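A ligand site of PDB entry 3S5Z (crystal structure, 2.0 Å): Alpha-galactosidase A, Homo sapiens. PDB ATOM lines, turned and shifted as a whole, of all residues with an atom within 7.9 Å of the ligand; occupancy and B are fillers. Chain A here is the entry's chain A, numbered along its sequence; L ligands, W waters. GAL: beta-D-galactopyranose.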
ATOM      1  N   THR A 215      -2.119  23.998  20.428  1.00  0.00           N
ATOM      2  CA  THR A 215      -2.863  23.631  19.264  1.00  0.00           C
ATOM      3  C   THR A 215      -3.796  24.683  18.707  1.00  0.00           C
ATOM      4  O   THR A 215      -3.877  24.814  17.476  1.00  0.00           O
ATOM      5  CB  THR A 215      -3.733  22.432  19.577  1.00  0.00           C
ATOM      6  OG1 THR A 215      -2.855  21.417  20.066  1.00  0.00           O
ATOM      7  CG2 THR A 215      -4.438  21.967  18.308  1.00  0.00           C
ATOM      8  N   SER A 216      -4.547  25.381  19.569  1.00  0.00           N
ATOM      9  CA  SER A 216      -5.418  26.420  19.076  1.00  0.00           C
ATOM     10  C   SER A 216      -4.527  27.590  18.626  1.00  0.00           C
ATOM     11  O   SER A 216      -4.777  28.226  17.627  1.00  0.00           O
ATOM     12  CB  SER A 216      -6.423  26.925  20.107  1.00  0.00           C
ATOM     13  OG  SER A 216      -5.838  27.204  21.360  1.00  0.00           O
ATOM     14  N   ASN A 218      -1.620  27.498  17.191  1.00  0.00           N
ATOM     15  CA  ASN A 218      -1.093  27.107  15.879  1.00  0.00           C
ATOM     16  C   ASN A 218      -2.073  26.461  14.897  1.00  0.00           C
ATOM     17  O   ASN A 218      -1.635  25.833  13.928  1.00  0.00           O
ATOM     18  CB  ASN A 218       0.068  26.133  16.096  1.00  0.00           C
ATOM     19  CG  ASN A 218       1.172  26.749  16.891  1.00  0.00           C
ATOM     20  OD1 ASN A 218       2.023  27.439  16.331  1.00  0.00           O
ATOM     21  ND2 ASN A 218       1.155  26.532  18.213  1.00  0.00           N
ATOM     22  N   GLN A 219      -3.376  26.608  15.123  1.00  0.00           N
ATOM     23  CA  GLN A 219      -4.342  25.850  14.328  1.00  0.00           C
ATOM     24  C   GLN A 219      -4.364  26.211  12.831  1.00  0.00           C
ATOM     25  O   GLN A 219      -4.649  25.368  11.999  1.00  0.00           O
ATOM     26  CB  GLN A 219      -5.745  25.903  14.931  1.00  0.00           C
ATOM     27  CG  GLN A 219      -6.432  27.233  14.954  1.00  0.00           C
ATOM     28  CD  GLN A 219      -7.830  27.166  15.525  1.00  0.00           C
ATOM     29  OE1 GLN A 219      -8.212  26.178  16.170  1.00  0.00           O
ATOM     30  NE2 GLN A 219      -8.620  28.203  15.279  1.00  0.00           N
ATOM     31  N   GLU A 220      -4.015  27.436  12.467  1.00  0.00           N
ATOM     32  CA  GLU A 220      -3.942  27.758  11.044  1.00  0.00           C
ATOM     33  C   GLU A 220      -2.917  26.862  10.339  1.00  0.00           C
ATOM     34  O   GLU A 220      -3.166  26.404   9.227  1.00  0.00           O
ATOM     35  CB  GLU A 220      -3.662  29.249  10.804  1.00  0.00           C
ATOM     36  CG  GLU A 220      -4.761  30.187  11.312  1.00  0.00           C
ATOM     37  CD  GLU A 220      -6.030  30.195  10.455  1.00  0.00           C
ATOM     38  OE1 GLU A 220      -6.409  29.138   9.909  1.00  0.00           O
ATOM     39  OE2 GLU A 220      -6.652  31.279  10.342  1.00  0.00           O
ATOM     40  N   ARG A 221      -1.783  26.587  10.998  1.00  0.00           N
ATOM     41  CA  ARG A 221      -0.717  25.785  10.390  1.00  0.00           C
ATOM     42  C   ARG A 221      -1.025  24.293  10.304  1.00  0.00           C
ATOM     43  O   ARG A 221      -0.520  23.613   9.415  1.00  0.00           O
ATOM     44  CB  ARG A 221       0.589  25.939  11.167  1.00  0.00           C
ATOM     45  CG  ARG A 221       1.208  27.328  11.126  1.00  0.00           C
ATOM     46  CD  ARG A 221       2.613  27.289  11.733  1.00  0.00           C
ATOM     47  NE  ARG A 221       3.492  28.297  11.132  1.00  0.00           N
ATOM     48  CZ  ARG A 221       3.764  29.488  11.662  1.00  0.00           C
ATOM     49  NH1 ARG A 221       3.254  29.871  12.825  1.00  0.00           N
ATOM     50  NH2 ARG A 221       4.582  30.314  11.002  1.00  0.00           N
ATOM     51  N   ILE A 222      -1.821  23.748  11.223  1.00  0.00           N
ATOM     52  CA  ILE A 222      -1.883  22.286  11.337  1.00  0.00           C
ATOM     53  C   ILE A 222      -3.244  21.616  11.076  1.00  0.00           C
ATOM     54  O   ILE A 222      -3.272  20.442  10.741  1.00  0.00           O
ATOM     55  CB  ILE A 222      -1.351  21.815  12.711  1.00  0.00           C
ATOM     56  CG1 ILE A 222      -2.269  22.230  13.854  1.00  0.00           C
ATOM     57  CG2 ILE A 222       0.052  22.320  12.962  1.00  0.00           C
ATOM     58  CD1 ILE A 222      -1.947  21.540  15.161  1.00  0.00           C
ATOM     59  N   VAL A 223      -4.354  22.338  11.248  1.00  0.00           N
ATOM     60  CA  VAL A 223      -5.663  21.686  11.196  1.00  0.00           C
ATOM     61  C   VAL A 223      -5.980  21.133   9.801  1.00  0.00           C
ATOM     62  O   VAL A 223      -6.469  20.011   9.661  1.00  0.00           O
ATOM     63  CB  VAL A 223      -6.782  22.617  11.732  1.00  0.00           C
ATOM     64  CG1 VAL A 223      -8.129  22.277  11.141  1.00  0.00           C
ATOM     65  CG2 VAL A 223      -6.874  22.530  13.257  1.00  0.00           C
ATOM     66  N   ASP A 224      -5.677  21.909   8.764  1.00  0.00           N
ATOM     67  CA  ASP A 224      -6.049  21.506   7.388  1.00  0.00           C
ATOM     68  C   ASP A 224      -5.165  20.404   6.792  1.00  0.00           C
ATOM     69  O   ASP A 224      -5.590  19.672   5.900  1.00  0.00           O
ATOM     70  CB  ASP A 224      -6.108  22.722   6.465  1.00  0.00           C
ATOM     71  CG  ASP A 224      -7.349  23.579   6.735  1.00  0.00           C
ATOM     72  OD1 ASP A 224      -8.372  23.040   7.208  1.00  0.00           O
ATOM     73  OD2 ASP A 224      -7.284  24.794   6.461  1.00  0.00           O
ATOM     74  N   VAL A 225      -3.952  20.252   7.327  1.00  0.00           N
ATOM     75  CA  VAL A 225      -3.069  19.169   6.903  1.00  0.00           C
ATOM     76  C   VAL A 225      -3.620  17.779   7.255  1.00  0.00           C
ATOM     77  O   VAL A 225      -3.370  16.813   6.540  1.00  0.00           O
ATOM     78  CB  VAL A 225      -1.685  19.287   7.554  1.00  0.00           C
ATOM     79  CG1 VAL A 225      -0.738  18.266   6.937  1.00  0.00           C
ATOM     80  CG2 VAL A 225      -1.131  20.709   7.401  1.00  0.00           C
ATOM     81  N   LYS A 295     -12.096  15.302   9.123  1.00  0.00           N
ATOM     82  CA  LYS A 295     -11.701  16.701   9.146  1.00  0.00           C
ATOM     83  C   LYS A 295     -11.425  17.114  10.586  1.00  0.00           C
ATOM     84  O   LYS A 295     -12.317  17.042  11.441  1.00  0.00           O
ATOM     85  CB  LYS A 295     -12.795  17.600   8.545  1.00  0.00           C
ATOM     86  CG  LYS A 295     -12.920  17.480   7.031  1.00  0.00           C
ATOM     87  CD  LYS A 295     -13.985  18.439   6.459  1.00  0.00           C
ATOM     88  CE  LYS A 295     -13.391  19.592   5.659  1.00  0.00           C
ATOM     89  NZ  LYS A 295     -12.123  20.110   6.244  1.00  0.00           N
ATOM     90  N   GLN A 296     -10.200  17.554  10.874  1.00  0.00           N
ATOM     91  CA  GLN A 296      -9.870  17.930  12.243  1.00  0.00           C
ATOM     92  C   GLN A 296     -10.719  19.146  12.645  1.00  0.00           C
ATOM     93  O   GLN A 296     -11.092  19.955  11.817  1.00  0.00           O
ATOM     94  CB  GLN A 296      -8.379  18.227  12.391  1.00  0.00           C
ATOM     95  CG  GLN A 296      -7.976  18.607  13.792  1.00  0.00           C
ATOM     96  CD  GLN A 296      -6.495  18.469  14.059  1.00  0.00           C
ATOM     97  OE1 GLN A 296      -5.804  17.657  13.424  1.00  0.00           O
ATOM     98  NE2 GLN A 296      -5.992  19.233  15.029  1.00  0.00           N
ATOM     99  N   GLY A 297     -11.031  19.252  13.933  1.00  0.00           N
ATOM    100  CA  GLY A 297     -11.771  20.365  14.468  1.00  0.00           C
ATOM    101  C   GLY A 297     -10.861  21.491  14.849  1.00  0.00           C
ATOM    102  O   GLY A 297      -9.657  21.421  14.613  1.00  0.00           O
ATOM    103  N   TYR A 298     -11.419  22.538  15.448  1.00  0.00           N
ATOM    104  CA  TYR A 298     -10.640  23.762  15.678  1.00  0.00           C
ATOM    105  C   TYR A 298     -11.342  24.610  16.728  1.00  0.00           C
ATOM    106  O   TYR A 298     -12.489  24.386  17.042  1.00  0.00           O
ATOM    107  CB  TYR A 298     -10.497  24.542  14.367  1.00  0.00           C
ATOM    108  CG  TYR A 298     -11.808  24.718  13.636  1.00  0.00           C
ATOM    109  CD1 TYR A 298     -12.656  25.787  13.937  1.00  0.00           C
ATOM    110  CD2 TYR A 298     -12.231  23.791  12.690  1.00  0.00           C
ATOM    111  CE1 TYR A 298     -13.875  25.944  13.290  1.00  0.00           C
ATOM    112  CE2 TYR A 298     -13.470  23.925  12.052  1.00  0.00           C
ATOM    113  CZ  TYR A 298     -14.279  25.009  12.357  1.00  0.00           C
ATOM    114  OH  TYR A 298     -15.496  25.164  11.732  1.00  0.00           O
ATOM    115  N   GLN A 299     -10.627  25.566  17.289  1.00  0.00           N
ATOM    116  CA  GLN A 299     -11.226  26.462  18.265  1.00  0.00           C
ATOM    117  C   GLN A 299     -11.928  27.556  17.480  1.00  0.00           C
ATOM    118  O   GLN A 299     -11.302  28.268  16.711  1.00  0.00           O
ATOM    119  CB  GLN A 299     -10.183  27.059  19.179  1.00  0.00           C
ATOM    120  CG  GLN A 299     -10.758  27.862  20.324  1.00  0.00           C
ATOM    121  CD  GLN A 299      -9.687  28.662  21.017  1.00  0.00           C
ATOM    122  OE1 GLN A 299      -9.208  29.643  20.484  1.00  0.00           O
ATOM    123  NE2 GLN A 299      -9.285  28.222  22.210  1.00  0.00           N
ATOM    124  N   LEU A 300     -13.236  27.677  17.696  1.00  0.00           N
ATOM    125  CA  LEU A 300     -14.070  28.699  17.066  1.00  0.00           C
ATOM    126  C   LEU A 300     -13.987  30.019  17.818  1.00  0.00           C
ATOM    127  O   LEU A 300     -13.896  31.083  17.200  1.00  0.00           O
ATOM    128  CB  LEU A 300     -15.528  28.218  17.043  1.00  0.00           C
ATOM    129  CG  LEU A 300     -16.566  29.226  16.552  1.00  0.00           C
ATOM    130  CD1 LEU A 300     -16.324  29.607  15.070  1.00  0.00           C
ATOM    131  CD2 LEU A 300     -17.952  28.642  16.780  1.00  0.00           C
ATOM    132  N   GLU A 310     -15.221  23.296  17.518  1.00  0.00           N
ATOM    133  CA  GLU A 310     -16.182  22.548  16.714  1.00  0.00           C
ATOM    134  C   GLU A 310     -15.514  21.632  15.680  1.00  0.00           C
ATOM    135  O   GLU A 310     -14.417  21.884  15.235  1.00  0.00           O
ATOM    136  CB  GLU A 310     -17.160  23.494  16.034  1.00  0.00           C
ATOM    137  CG  GLU A 310     -16.578  24.386  14.958  1.00  0.00           C
ATOM    138  CD  GLU A 310     -17.620  25.268  14.296  1.00  0.00           C
ATOM    139  OE1 GLU A 310     -17.363  25.991  13.380  1.00  0.00           O
ATOM    140  OE2 GLU A 310     -18.763  25.279  14.656  1.00  0.00           O
ATOM    141  N   PRO A 312     -16.477  19.463  11.951  1.00  0.00           N
ATOM    142  CA  PRO A 312     -17.390  18.990  10.929  1.00  0.00           C
ATOM    143  C   PRO A 312     -17.365  17.464  10.785  1.00  0.00           C
ATOM    144  O   PRO A 312     -16.300  16.880  10.716  1.00  0.00           O
ATOM    145  CB  PRO A 312     -16.880  19.664   9.653  1.00  0.00           C
ATOM    146  CG  PRO A 312     -15.488  19.942   9.899  1.00  0.00           C
ATOM    147  CD  PRO A 312     -15.286  20.111  11.372  1.00  0.00           C
ATOM    148  N   TRP A 318     -22.319  18.018  13.040  1.00  0.00           N
ATOM    149  CA  TRP A 318     -21.218  18.748  13.679  1.00  0.00           C
ATOM    150  C   TRP A 318     -21.072  18.329  15.128  1.00  0.00           C
ATOM    151  O   TRP A 318     -22.058  17.987  15.791  1.00  0.00           O
ATOM    152  CB  TRP A 318     -21.460  20.255  13.617  1.00  0.00           C
ATOM    153  CG  TRP A 318     -21.339  20.822  12.253  1.00  0.00           C
ATOM    154  CD1 TRP A 318     -22.271  20.757  11.237  1.00  0.00           C
ATOM    155  CD2 TRP A 318     -20.218  21.541  11.721  1.00  0.00           C
ATOM    156  NE1 TRP A 318     -21.784  21.382  10.122  1.00  0.00           N
ATOM    157  CE2 TRP A 318     -20.534  21.872  10.389  1.00  0.00           C
ATOM    158  CE3 TRP A 318     -18.988  21.931  12.240  1.00  0.00           C
ATOM    159  CZ2 TRP A 318     -19.656  22.571   9.567  1.00  0.00           C
ATOM    160  CZ3 TRP A 318     -18.115  22.637  11.424  1.00  0.00           C
ATOM    161  CH2 TRP A 318     -18.461  22.956  10.097  1.00  0.00           C
ATOM    162  N   LYS A 343     -20.202  27.334  10.616  1.00  0.00           N
ATOM    163  CA  LYS A 343     -20.170  28.436   9.666  1.00  0.00           C
ATOM    164  C   LYS A 343     -21.564  28.911   9.217  1.00  0.00           C
ATOM    165  O   LYS A 343     -21.741  29.391   8.110  1.00  0.00           O
ATOM    166  CB  LYS A 343     -19.299  28.063   8.455  1.00  0.00           C
ATOM    167  CG  LYS A 343     -17.822  27.931   8.808  1.00  0.00           C
ATOM    168  CD  LYS A 343     -16.960  27.761   7.553  1.00  0.00           C
ATOM    169  CE  LYS A 343     -15.481  27.803   7.891  1.00  0.00           C
ATOM    170  NZ  LYS A 343     -15.098  26.758   8.887  1.00  0.00           N
HETATM  171  C1  GAL L   1     -11.854  27.341  10.089  1.00  0.00           C
HETATM  172  C2  GAL L   1     -11.479  26.389   8.951  1.00  0.00           C
HETATM  173  C3  GAL L   1     -10.594  25.268   9.470  1.00  0.00           C
HETATM  174  C4  GAL L   1      -9.395  25.813  10.245  1.00  0.00           C
HETATM  175  C5  GAL L   1      -9.830  26.888  11.252  1.00  0.00           C
HETATM  176  C6  GAL L   1      -8.657  27.575  11.926  1.00  0.00           C
HETATM  177  O1  GAL L   1     -12.669  28.422   9.617  1.00  0.00           O
HETATM  178  O2  GAL L   1     -12.671  25.822   8.372  1.00  0.00           O
HETATM  179  O3  GAL L   1     -10.161  24.452   8.372  1.00  0.00           O
HETATM  180  O4  GAL L   1      -8.408  26.326   9.333  1.00  0.00           O
HETATM  181  O5  GAL L   1     -10.646  27.871  10.633  1.00  0.00           O
HETATM  182  O6  GAL L   1      -9.073  28.843  12.458  1.00  0.00           O
HETATM  183  O   HOH W   1      -7.371  30.369  13.732  1.00  0.00           O
HETATM  184  O   HOH W   2     -13.589  22.850   8.400  1.00  0.00           O
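NZ of Lys 343 lies within hydrogen-bond range of OH of Tyr 298 (3.3 Å). The backbone NH (N) of Gln 299 lies within hydrogen-bond range of the side-chain amide oxygen (OE1) of Gln 219, at 2.7 Å. The side-chain hydroxyl (OH) of Tyr 298 is in hydrogen-bond range of the side-chain carboxylate (OE1) of Glu 310, at 2.6 Å.
Water W1 lies within hydrogen-bond range of an oxygen (O6) of the ligand and the side-chain amide nitrogen (NE2) of Gln 219.
Merely in contact with the ligand: Val 223 (3.9 Å) and Tyr 298 (3.8 Å). Six residues have an atom within 4 Å of the ligand: Gln 219, Glu 220, Val 223, Asp 224, Tyr 298 and Lys 343. The nearest printed residue that does not touch the ligand is Gln 299 (4.8 Å).
The side-chain carboxylate (OD1) of Asp 224 is in hydrogen-bond range of an oxygen (O3) of the ligand, 2.6 Å away. An oxygen (O2) of the ligand is in hydrogen-bond range of the side-chain amino group (NZ) of Lys 343. NE2 of Gln 219 is in hydrogen-bond range of O6 of the ligand, at 2.9 Å. The side-chain carboxylate (OE1) of Glu 220 lies close to an oxygen (O4) of the ligand (3.5 Å).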
